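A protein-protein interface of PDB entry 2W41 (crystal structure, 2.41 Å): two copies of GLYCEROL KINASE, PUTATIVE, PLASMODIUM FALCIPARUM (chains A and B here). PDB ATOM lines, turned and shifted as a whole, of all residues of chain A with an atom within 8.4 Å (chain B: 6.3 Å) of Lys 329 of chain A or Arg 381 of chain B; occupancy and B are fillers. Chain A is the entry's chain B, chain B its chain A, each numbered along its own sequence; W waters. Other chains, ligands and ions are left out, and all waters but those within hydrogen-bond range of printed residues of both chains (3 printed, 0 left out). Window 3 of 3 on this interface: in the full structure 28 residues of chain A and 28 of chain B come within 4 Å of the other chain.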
ATOM      1  N   VAL A 322      13.675 -25.312 -27.651  1.00  0.00           N
ATOM      2  CA  VAL A 322      12.978 -25.759 -26.445  1.00  0.00           C
ATOM      3  C   VAL A 322      13.942 -26.210 -25.326  1.00  0.00           C
ATOM      4  O   VAL A 322      13.679 -25.937 -24.157  1.00  0.00           O
ATOM      5  CB  VAL A 322      11.939 -26.841 -26.721  1.00  0.00           C
ATOM      6  CG1 VAL A 322      11.327 -27.271 -25.411  1.00  0.00           C
ATOM      7  CG2 VAL A 322      10.853 -26.340 -27.663  1.00  0.00           C
ATOM      8  N   SER A 323      15.049 -26.871 -25.665  1.00  0.00           N
ATOM      9  CA  SER A 323      16.124 -27.099 -24.690  1.00  0.00           C
ATOM     10  C   SER A 323      16.755 -25.813 -24.115  1.00  0.00           C
ATOM     11  O   SER A 323      17.123 -25.776 -22.924  1.00  0.00           O
ATOM     12  CB  SER A 323      17.253 -27.973 -25.281  1.00  0.00           C
ATOM     13  OG  SER A 323      16.752 -28.832 -26.294  1.00  0.00           O
ATOM     14  N   TRP A 324      16.915 -24.799 -24.956  1.00  0.00           N
ATOM     15  CA  TRP A 324      17.471 -23.498 -24.561  1.00  0.00           C
ATOM     16  C   TRP A 324      16.543 -22.710 -23.567  1.00  0.00           C
ATOM     17  O   TRP A 324      17.005 -22.087 -22.602  1.00  0.00           O
ATOM     18  CB  TRP A 324      17.806 -22.684 -25.841  1.00  0.00           C
ATOM     19  CG  TRP A 324      18.365 -21.322 -25.625  1.00  0.00           C
ATOM     20  CD1 TRP A 324      19.670 -20.965 -25.679  1.00  0.00           C
ATOM     21  CD2 TRP A 324      17.628 -20.118 -25.346  1.00  0.00           C
ATOM     22  NE1 TRP A 324      19.810 -19.617 -25.423  1.00  0.00           N
ATOM     23  CE2 TRP A 324      18.565 -19.077 -25.205  1.00  0.00           C
ATOM     24  CE3 TRP A 324      16.254 -19.818 -25.176  1.00  0.00           C
ATOM     25  CZ2 TRP A 324      18.181 -17.768 -24.909  1.00  0.00           C
ATOM     26  CZ3 TRP A 324      15.887 -18.501 -24.842  1.00  0.00           C
ATOM     27  CH2 TRP A 324      16.835 -17.507 -24.736  1.00  0.00           C
ATOM     28  N   LEU A 325      15.237 -22.755 -23.786  1.00  0.00           N
ATOM     29  CA  LEU A 325      14.279 -22.257 -22.791  1.00  0.00           C
ATOM     30  C   LEU A 325      14.484 -22.954 -21.440  1.00  0.00           C
ATOM     31  O   LEU A 325      14.462 -22.294 -20.396  1.00  0.00           O
ATOM     32  CB  LEU A 325      12.824 -22.418 -23.291  1.00  0.00           C
ATOM     33  CG  LEU A 325      12.452 -21.751 -24.632  1.00  0.00           C
ATOM     34  CD1 LEU A 325      11.055 -22.183 -25.177  1.00  0.00           C
ATOM     35  CD2 LEU A 325      12.595 -20.224 -24.531  1.00  0.00           C
ATOM     36  N   LEU A 326      14.688 -24.277 -21.482  1.00  0.00           N
ATOM     37  CA  LEU A 326      14.976 -25.108 -20.297  1.00  0.00           C
ATOM     38  C   LEU A 326      16.344 -24.809 -19.613  1.00  0.00           C
ATOM     39  O   LEU A 326      16.444 -24.778 -18.396  1.00  0.00           O
ATOM     40  CB  LEU A 326      14.930 -26.596 -20.657  1.00  0.00           C
ATOM     41  CG  LEU A 326      13.634 -27.395 -20.738  1.00  0.00           C
ATOM     42  CD1 LEU A 326      13.935 -28.734 -21.302  1.00  0.00           C
ATOM     43  CD2 LEU A 326      13.016 -27.613 -19.386  1.00  0.00           C
ATOM     44  N   LYS A 327      17.396 -24.608 -20.389  1.00  0.00           N
ATOM     45  CA  LYS A 327      18.645 -24.118 -19.791  1.00  0.00           C
ATOM     46  C   LYS A 327      18.475 -22.755 -19.104  1.00  0.00           C
ATOM     47  O   LYS A 327      19.038 -22.517 -18.067  1.00  0.00           O
ATOM     48  CB  LYS A 327      19.778 -24.070 -20.820  1.00  0.00           C
ATOM     49  CG  LYS A 327      21.034 -23.439 -20.298  1.00  0.00           C
ATOM     50  CD  LYS A 327      22.140 -23.572 -21.284  1.00  0.00           C
ATOM     51  CE  LYS A 327      21.879 -22.801 -22.582  1.00  0.00           C
ATOM     52  NZ  LYS A 327      22.796 -23.316 -23.657  1.00  0.00           N
ATOM     53  N   ASN A 328      17.676 -21.873 -19.673  1.00  0.00           N
ATOM     54  CA  ASN A 328      17.528 -20.527 -19.116  1.00  0.00           C
ATOM     55  C   ASN A 328      16.343 -20.387 -18.190  1.00  0.00           C
ATOM     56  O   ASN A 328      15.994 -19.259 -17.818  1.00  0.00           O
ATOM     57  CB  ASN A 328      17.561 -19.472 -20.229  1.00  0.00           C
ATOM     58  CG  ASN A 328      18.882 -19.462 -20.901  1.00  0.00           C
ATOM     59  OD1 ASN A 328      19.017 -19.444 -22.109  1.00  0.00           O
ATOM     60  ND2 ASN A 328      19.892 -19.607 -20.094  1.00  0.00           N
ATOM     61  N   LYS A 329      15.764 -21.542 -17.818  1.00  0.00           N
ATOM     62  CA  LYS A 329      14.783 -21.662 -16.728  1.00  0.00           C
ATOM     63  C   LYS A 329      13.476 -21.051 -17.131  1.00  0.00           C
ATOM     64  O   LYS A 329      12.591 -20.897 -16.311  1.00  0.00           O
ATOM     65  CB  LYS A 329      15.267 -21.017 -15.411  1.00  0.00           C
ATOM     66  CG  LYS A 329      16.563 -21.541 -14.813  1.00  0.00           C
ATOM     67  CD  LYS A 329      16.382 -22.985 -14.336  1.00  0.00           C
ATOM     68  CE  LYS A 329      17.727 -23.625 -13.938  1.00  0.00           C
ATOM     69  NZ  LYS A 329      17.710 -25.104 -14.211  1.00  0.00           N
ATOM     70  N   LEU A 330      13.340 -20.728 -18.412  1.00  0.00           N
ATOM     71  CA  LEU A 330      12.079 -20.168 -18.933  1.00  0.00           C
ATOM     72  C   LEU A 330      10.904 -21.157 -19.008  1.00  0.00           C
ATOM     73  O   LEU A 330       9.774 -20.720 -19.199  1.00  0.00           O
ATOM     74  CB  LEU A 330      12.308 -19.484 -20.282  1.00  0.00           C
ATOM     75  CG  LEU A 330      13.194 -18.240 -20.251  1.00  0.00           C
ATOM     76  CD1 LEU A 330      13.895 -18.084 -21.533  1.00  0.00           C
ATOM     77  CD2 LEU A 330      12.368 -17.038 -19.953  1.00  0.00           C
ATOM     78  N   ILE A 331      11.202 -22.460 -18.898  1.00  0.00           N
ATOM     79  CA  ILE A 331      10.240 -23.560 -18.646  1.00  0.00           C
ATOM     80  C   ILE A 331      10.919 -24.634 -17.821  1.00  0.00           C
ATOM     81  O   ILE A 331      12.153 -24.756 -17.836  1.00  0.00           O
ATOM     82  CB  ILE A 331       9.710 -24.281 -19.924  1.00  0.00           C
ATOM     83  CG1 ILE A 331      10.849 -24.639 -20.892  1.00  0.00           C
ATOM     84  CG2 ILE A 331       8.650 -23.462 -20.575  1.00  0.00           C
ATOM     85  CD1 ILE A 331      10.429 -25.447 -22.024  1.00  0.00           C
ATOM     86  N   ASP A 332      10.130 -25.437 -17.121  1.00  0.00           N
ATOM     87  CA  ASP A 332      10.704 -26.520 -16.292  1.00  0.00           C
ATOM     88  C   ASP A 332      10.749 -27.922 -16.927  1.00  0.00           C
ATOM     89  O   ASP A 332      11.557 -28.771 -16.507  1.00  0.00           O
ATOM     90  CB  ASP A 332      10.020 -26.572 -14.931  1.00  0.00           C
ATOM     91  CG  ASP A 332      10.521 -25.482 -14.003  1.00  0.00           C
ATOM     92  OD1 ASP A 332      10.543 -24.284 -14.432  1.00  0.00           O
ATOM     93  OD2 ASP A 332      10.906 -25.835 -12.846  1.00  0.00           O
ATOM     94  N   ASP A 333       9.895 -28.142 -17.928  1.00  0.00           N
ATOM     95  CA  ASP A 333       9.744 -29.415 -18.605  1.00  0.00           C
ATOM     96  C   ASP A 333       9.168 -29.099 -19.977  1.00  0.00           C
ATOM     97  O   ASP A 333       8.356 -28.204 -20.096  1.00  0.00           O
ATOM     98  CB  ASP A 333       8.752 -30.321 -17.849  1.00  0.00           C
ATOM     99  CG  ASP A 333       8.619 -31.720 -18.480  1.00  0.00           C
ATOM    100  OD1 ASP A 333       9.601 -32.511 -18.345  1.00  0.00           O
ATOM    101  OD2 ASP A 333       7.561 -32.025 -19.117  1.00  0.00           O
ATOM    102  N   GLU A 336       5.405 -28.499 -20.324  1.00  0.00           N
ATOM    103  CA  GLU A 336       4.997 -27.143 -19.984  1.00  0.00           C
ATOM    104  C   GLU A 336       4.859 -26.233 -21.215  1.00  0.00           C
ATOM    105  O   GLU A 336       4.200 -25.205 -21.145  1.00  0.00           O
ATOM    106  CB  GLU A 336       6.011 -26.560 -19.023  1.00  0.00           C
ATOM    107  CG  GLU A 336       5.550 -25.399 -18.150  1.00  0.00           C
ATOM    108  CD  GLU A 336       6.720 -24.795 -17.357  1.00  0.00           C
ATOM    109  OE1 GLU A 336       7.507 -25.587 -16.774  1.00  0.00           O
ATOM    110  OE2 GLU A 336       6.876 -23.547 -17.340  1.00  0.00           O
ATOM    111  N   ARG A 381       7.394 -15.455 -18.826  1.00  0.00           N
ATOM    112  CA  ARG A 381       7.998 -16.678 -19.406  1.00  0.00           C
ATOM    113  C   ARG A 381       7.120 -17.230 -20.578  1.00  0.00           C
ATOM    114  O   ARG A 381       7.648 -17.544 -21.666  1.00  0.00           O
ATOM    115  CB  ARG A 381       8.174 -17.784 -18.348  1.00  0.00           C
ATOM    116  CG  ARG A 381       9.258 -17.583 -17.317  1.00  0.00           C
ATOM    117  CD  ARG A 381       9.428 -18.814 -16.412  1.00  0.00           C
ATOM    118  NE  ARG A 381       8.180 -19.169 -15.717  1.00  0.00           N
ATOM    119  CZ  ARG A 381       7.378 -20.203 -16.029  1.00  0.00           C
ATOM    120  NH1 ARG A 381       7.692 -21.047 -17.004  1.00  0.00           N
ATOM    121  NH2 ARG A 381       6.237 -20.404 -15.361  1.00  0.00           N
ATOM    122  N   VAL A 385       8.236 -17.996 -24.510  1.00  0.00           N
ATOM    123  CA  VAL A 385       8.160 -19.414 -24.874  1.00  0.00           C
ATOM    124  C   VAL A 385       7.240 -19.599 -26.079  1.00  0.00           C
ATOM    125  O   VAL A 385       7.619 -20.252 -27.048  1.00  0.00           O
ATOM    126  CB  VAL A 385       7.643 -20.310 -23.702  1.00  0.00           C
ATOM    127  CG1 VAL A 385       7.292 -21.692 -24.206  1.00  0.00           C
ATOM    128  CG2 VAL A 385       8.677 -20.448 -22.584  1.00  0.00           C
ATOM    129  N   ASN B 328      10.860 -13.831 -14.617  1.00  0.00           N
ATOM    130  CA  ASN B 328      11.070 -14.792 -15.716  1.00  0.00           C
ATOM    131  C   ASN B 328      12.116 -15.858 -15.399  1.00  0.00           C
ATOM    132  O   ASN B 328      12.479 -16.654 -16.275  1.00  0.00           O
ATOM    133  CB  ASN B 328      11.295 -14.063 -17.058  1.00  0.00           C
ATOM    134  CG  ASN B 328      10.090 -13.283 -17.440  1.00  0.00           C
ATOM    135  OD1 ASN B 328      10.129 -12.127 -17.802  1.00  0.00           O
ATOM    136  ND2 ASN B 328       8.967 -13.895 -17.204  1.00  0.00           N
ATOM    137  N   LYS B 329      12.555 -15.872 -14.132  1.00  0.00           N
ATOM    138  CA  LYS B 329      13.309 -16.967 -13.531  1.00  0.00           C
ATOM    139  C   LYS B 329      14.718 -16.914 -14.017  1.00  0.00           C
ATOM    140  O   LYS B 329      15.510 -17.836 -13.797  1.00  0.00           O
ATOM    141  CB  LYS B 329      12.695 -18.348 -13.843  1.00  0.00           C
ATOM    142  CG  LYS B 329      11.250 -18.577 -13.361  1.00  0.00           C
ATOM    143  CD  LYS B 329      11.216 -18.636 -11.835  1.00  0.00           C
ATOM    144  CE  LYS B 329       9.784 -18.682 -11.294  1.00  0.00           C
ATOM    145  NZ  LYS B 329       9.734 -17.960  -9.993  1.00  0.00           N
ATOM    146  N   LEU B 330      15.051 -15.811 -14.675  1.00  0.00           N
ATOM    147  CA  LEU B 330      16.415 -15.632 -15.199  1.00  0.00           C
ATOM    148  C   LEU B 330      17.480 -15.390 -14.118  1.00  0.00           C
ATOM    149  O   LEU B 330      18.649 -15.473 -14.414  1.00  0.00           O
ATOM    150  CB  LEU B 330      16.438 -14.531 -16.263  1.00  0.00           C
ATOM    151  CG  LEU B 330      15.723 -14.903 -17.558  1.00  0.00           C
ATOM    152  CD1 LEU B 330      15.218 -13.655 -18.203  1.00  0.00           C
ATOM    153  CD2 LEU B 330      16.670 -15.654 -18.461  1.00  0.00           C
ATOM    154  N   ILE B 331      17.036 -15.065 -12.898  1.00  0.00           N
ATOM    155  CA  ILE B 331      17.816 -15.064 -11.640  1.00  0.00           C
ATOM    156  C   ILE B 331      16.898 -15.454 -10.500  1.00  0.00           C
ATOM    157  O   ILE B 331      15.678 -15.274 -10.574  1.00  0.00           O
ATOM    158  CB  ILE B 331      18.442 -13.685 -11.256  1.00  0.00           C
ATOM    159  CG1 ILE B 331      17.454 -12.539 -11.407  1.00  0.00           C
ATOM    160  CG2 ILE B 331      19.721 -13.447 -12.033  1.00  0.00           C
ATOM    161  CD1 ILE B 331      17.951 -11.281 -10.870  1.00  0.00           C
ATOM    162  N   ASP B 332      17.473 -15.964  -9.425  1.00  0.00           N
ATOM    163  CA  ASP B 332      16.666 -16.339  -8.232  1.00  0.00           C
ATOM    164  C   ASP B 332      16.603 -15.307  -7.087  1.00  0.00           C
ATOM    165  O   ASP B 332      15.657 -15.338  -6.282  1.00  0.00           O
ATOM    166  CB  ASP B 332      17.116 -17.694  -7.705  1.00  0.00           C
ATOM    167  CG  ASP B 332      16.589 -18.835  -8.555  1.00  0.00           C
ATOM    168  OD1 ASP B 332      16.753 -18.806  -9.822  1.00  0.00           O
ATOM    169  OD2 ASP B 332      15.980 -19.764  -7.950  1.00  0.00           O
ATOM    170  N   GLU B 336      22.282 -12.496  -6.748  1.00  0.00           N
ATOM    171  CA  GLU B 336      22.789 -13.262  -7.876  1.00  0.00           C
ATOM    172  C   GLU B 336      23.228 -12.385  -9.072  1.00  0.00           C
ATOM    173  O   GLU B 336      23.959 -12.858  -9.940  1.00  0.00           O
ATOM    174  CB  GLU B 336      21.708 -14.221  -8.312  1.00  0.00           C
ATOM    175  CG  GLU B 336      22.149 -15.474  -9.072  1.00  0.00           C
ATOM    176  CD  GLU B 336      20.938 -16.295  -9.564  1.00  0.00           C
ATOM    177  OE1 GLU B 336      19.980 -16.519  -8.780  1.00  0.00           O
ATOM    178  OE2 GLU B 336      20.930 -16.706 -10.741  1.00  0.00           O
ATOM    179  N   ILE B 340      26.849 -12.832 -10.942  1.00  0.00           N
ATOM    180  CA  ILE B 340      26.849 -12.990 -12.389  1.00  0.00           C
ATOM    181  C   ILE B 340      27.811 -12.020 -13.082  1.00  0.00           C
ATOM    182  O   ILE B 340      28.541 -12.423 -13.973  1.00  0.00           O
ATOM    183  CB  ILE B 340      25.398 -12.914 -12.928  1.00  0.00           C
ATOM    184  CG1 ILE B 340      24.683 -14.244 -12.618  1.00  0.00           C
ATOM    185  CG2 ILE B 340      25.347 -12.461 -14.392  1.00  0.00           C
ATOM    186  CD1 ILE B 340      23.148 -14.317 -12.946  1.00  0.00           C
ATOM    187  N   THR B 379      24.245 -18.967 -25.516  1.00  0.00           N
ATOM    188  CA  THR B 379      23.732 -17.965 -24.566  1.00  0.00           C
ATOM    189  C   THR B 379      23.001 -18.526 -23.290  1.00  0.00           C
ATOM    190  O   THR B 379      22.138 -19.424 -23.369  1.00  0.00           O
ATOM    191  CB  THR B 379      22.850 -16.911 -25.316  1.00  0.00           C
ATOM    192  OG1 THR B 379      23.626 -16.292 -26.370  1.00  0.00           O
ATOM    193  CG2 THR B 379      22.289 -15.842 -24.346  1.00  0.00           C
ATOM    194  N   GLU B 380      23.342 -17.952 -22.129  1.00  0.00           N
ATOM    195  CA  GLU B 380      22.883 -18.435 -20.831  1.00  0.00           C
ATOM    196  C   GLU B 380      22.246 -17.335 -20.005  1.00  0.00           C
ATOM    197  O   GLU B 380      22.471 -16.167 -20.320  1.00  0.00           O
ATOM    198  CB  GLU B 380      24.097 -18.919 -20.070  1.00  0.00           C
ATOM    199  CG  GLU B 380      24.672 -20.227 -20.585  1.00  0.00           C
ATOM    200  CD  GLU B 380      25.491 -20.947 -19.510  1.00  0.00           C
ATOM    201  OE1 GLU B 380      25.638 -20.359 -18.412  1.00  0.00           O
ATOM    202  OE2 GLU B 380      25.950 -22.098 -19.755  1.00  0.00           O
ATOM    203  N   ARG B 381      21.506 -17.686 -18.933  1.00  0.00           N
ATOM    204  CA  ARG B 381      20.869 -16.688 -18.035  1.00  0.00           C
ATOM    205  C   ARG B 381      21.877 -15.563 -17.740  1.00  0.00           C
ATOM    206  O   ARG B 381      21.534 -14.367 -17.873  1.00  0.00           O
ATOM    207  CB  ARG B 381      20.387 -17.298 -16.698  1.00  0.00           C
ATOM    208  CG  ARG B 381      19.217 -18.244 -16.771  1.00  0.00           C
ATOM    209  CD  ARG B 381      18.783 -18.834 -15.399  1.00  0.00           C
ATOM    210  NE  ARG B 381      19.869 -19.485 -14.657  1.00  0.00           N
ATOM    211  CZ  ARG B 381      20.560 -18.939 -13.635  1.00  0.00           C
ATOM    212  NH1 ARG B 381      20.286 -17.717 -13.164  1.00  0.00           N
ATOM    213  NH2 ARG B 381      21.562 -19.616 -13.071  1.00  0.00           N
ATOM    214  N   SER B 382      23.104 -15.954 -17.367  1.00  0.00           N
ATOM    215  CA  SER B 382      24.240 -15.049 -17.150  1.00  0.00           C
ATOM    216  C   SER B 382      24.451 -13.933 -18.126  1.00  0.00           C
ATOM    217  O   SER B 382      24.795 -12.787 -17.724  1.00  0.00           O
ATOM    218  CB  SER B 382      25.576 -15.824 -17.146  1.00  0.00           C
ATOM    219  OG  SER B 382      25.888 -16.220 -15.838  1.00  0.00           O
ATOM    220  N   HIS B 383      24.362 -14.288 -19.410  1.00  0.00           N
ATOM    221  CA  HIS B 383      24.683 -13.349 -20.507  1.00  0.00           C
ATOM    222  C   HIS B 383      23.580 -12.331 -20.668  1.00  0.00           C
ATOM    223  O   HIS B 383      23.826 -11.174 -20.983  1.00  0.00           O
ATOM    224  CB  HIS B 383      24.855 -14.100 -21.808  1.00  0.00           C
ATOM    225  CG  HIS B 383      25.938 -15.133 -21.784  1.00  0.00           C
ATOM    226  ND1 HIS B 383      27.272 -14.815 -21.888  1.00  0.00           N
ATOM    227  CD2 HIS B 383      25.882 -16.482 -21.735  1.00  0.00           C
ATOM    228  CE1 HIS B 383      27.995 -15.920 -21.863  1.00  0.00           C
ATOM    229  NE2 HIS B 383      27.175 -16.947 -21.777  1.00  0.00           N
ATOM    230  N   ILE B 384      22.350 -12.791 -20.446  1.00  0.00           N
ATOM    231  CA  ILE B 384      21.136 -11.992 -20.649  1.00  0.00           C
ATOM    232  C   ILE B 384      20.990 -11.000 -19.513  1.00  0.00           C
ATOM    233  O   ILE B 384      20.627  -9.846 -19.757  1.00  0.00           O
ATOM    234  CB  ILE B 384      19.896 -12.915 -20.700  1.00  0.00           C
ATOM    235  CG1 ILE B 384      19.903 -13.740 -21.982  1.00  0.00           C
ATOM    236  CG2 ILE B 384      18.559 -12.113 -20.459  1.00  0.00           C
ATOM    237  CD1 ILE B 384      19.045 -14.992 -21.894  1.00  0.00           C
ATOM    238  N   VAL B 385      21.239 -11.483 -18.285  1.00  0.00           N
ATOM    239  CA  VAL B 385      21.222 -10.695 -17.033  1.00  0.00           C
ATOM    240  C   VAL B 385      22.302  -9.618 -17.099  1.00  0.00           C
ATOM    241  O   VAL B 385      22.014  -8.451 -16.841  1.00  0.00           O
ATOM    242  CB  VAL B 385      21.445 -11.576 -15.761  1.00  0.00           C
ATOM    243  CG1 VAL B 385      21.741 -10.735 -14.534  1.00  0.00           C
ATOM    244  CG2 VAL B 385      20.272 -12.476 -15.471  1.00  0.00           C
ATOM    245  N   ARG B 386      23.533  -9.988 -17.446  1.00  0.00           N
ATOM    246  CA  ARG B 386      24.579  -8.982 -17.638  1.00  0.00           C
ATOM    247  C   ARG B 386      24.244  -7.889 -18.730  1.00  0.00           C
ATOM    248  O   ARG B 386      24.461  -6.653 -18.504  1.00  0.00           O
ATOM    249  CB  ARG B 386      25.934  -9.662 -17.886  1.00  0.00           C
ATOM    250  CG  ARG B 386      27.030  -8.688 -18.200  1.00  0.00           C
ATOM    251  CD  ARG B 386      28.465  -9.210 -18.237  1.00  0.00           C
ATOM    252  NE  ARG B 386      29.248  -7.988 -18.382  1.00  0.00           N
ATOM    253  CZ  ARG B 386      30.088  -7.469 -17.490  1.00  0.00           C
ATOM    254  NH1 ARG B 386      30.370  -8.123 -16.375  1.00  0.00           N
ATOM    255  NH2 ARG B 386      30.661  -6.290 -17.736  1.00  0.00           N
HETATM  256  O   HOH W   1      21.488 -21.057 -18.104  1.00  0.00           O
HETATM  257  O   HOH W   2      25.778 -22.439 -22.279  1.00  0.00           O
HETATM  258  O   HOH W   3       6.861 -15.290 -15.515  1.00  0.00           O
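ND2 of Asn 328 of chain B sits close to N of Arg 381 of chain A, at 2.7 Å.
The backbone carbonyl oxygen of Thr 379 of chain B sits at hydrogen-bond distance from the indole nitrogen of Trp 324 of chain A (3.1 Å).
O of Thr 379 of chain B lies close to OD1 of Asn 328 of chain A.
N of Arg 381 of chain B lies close to ND2 of Asn 328 of chain A (2.8 Å).
The backbone carbonyl oxygen (O) of Leu 330 of chain B is in hydrogen-bond range of the guanidinium group (NH1) of Arg 381 of chain B.
NH1 of Arg 381 of chain B is in salt-bridge range of OE2 of Glu 336 of chain B, 2.7 Å away.
O of Trp 324 of chain A lies close to OD1 of Asn 328 of chain A (3.4 Å).
N of Leu 330 of chain A is in hydrogen-bond range of O of Leu 325 of chain A, 2.8 Å away.
O of Leu 330 of chain A is in hydrogen-bond range of NH1 of Arg 381 of chain A (3.0 Å).
The side-chain carboxylate (OE2) of Glu 336 of chain A lies within salt-bridge range of the guanidinium group (NH1) of Arg 381 of chain A (2.7 Å).
Among the printed residues, pairs that only touch across the chains: Lys 327 of chain A with Thr 379 of chain B (3.5 Å), Asn 328 of chain A with Leu 330 of chain B (3.7 Å), Asn 328 of chain A with Glu 380 of chain B (3.3 Å), Lys 329 of chain A with Lys 329 of chain B (3.5 Å), Lys 329 of chain A with Arg 381 of chain B (3.5 Å), Leu 330 of chain A with Asn 328 of chain B (3.7 Å) and Arg 381 of chain A with Lys 329 of chain B (3.6 Å).
Leu 326 of chain A touches none of the printed residues of chain B.
Of the printed residues of chain B, Lys 327 of chain A touches Thr 379 (3.5 Å).
Of the printed residues of chain B, Asn 328 of chain A touches Leu 330 (3.7 Å), Thr 379 (3.4 Å), Glu 380 (3.3 Å) and Arg 381 (2.8 Å).
Lys 329 of chain A touches just these residues of chain B: Lys 329 and Arg 381.
Of the printed residues of chain A, Thr 379 of chain B touches Trp 324, Lys 327 and Asn 328.
Arg 381 of chain B touches just these residues of chain A: Asn 328 and Lys 329.
Arg 386 of chain B touches none of the printed residues of chain A.
The nearest printed residue of chain B that does not touch Lys 327 of chain A is Glu 380 of chain B (4.3 Å).
Of the 15 printed residues of chain A, 6 touch a printed residue of chain B.
Among the printed residues, 11 pairs touch across the chains.
Asn 328 of chain A touches Leu 330 of chain B, and with the chains exchanged Leu 330 of chain A touches Asn 328 of chain B.
Asn 328 of chain A touches Arg 381 of chain B, and with the chains exchanged Arg 381 of chain A touches Asn 328 of chain B.
Lys 329 of chain A touches its own counterpart, Lys 329 of chain B.
Lys 329 of chain A touches Arg 381 of chain B, and with the chains exchanged Arg 381 of chain A touches Lys 329 of chain B.
8 positions are printed for both chains.
Of the 11 pairs that touch across the chains among the printed residues, 7 have their exchanged pair printed and touching as well.
Water W2 lies within hydrogen-bond range of OE2 of Glu 380 of chain B (2.6 Å) and NZ of Lys 327 of chain A (3.4 Å).
Water W1 lies within hydrogen-bond range of O of Lys 327 of chain A (2.9 Å), ND2 of Asn 328 of chain A (2.9 Å) and N of Arg 381 of chain B (3.5 Å).
Water W3 lies within hydrogen-bond range of the side-chain amide nitrogen (ND2) of Asn 328 of chain B (3.0 Å) and the backbone NH (N) of Arg 381 of chain A (3.4 Å).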
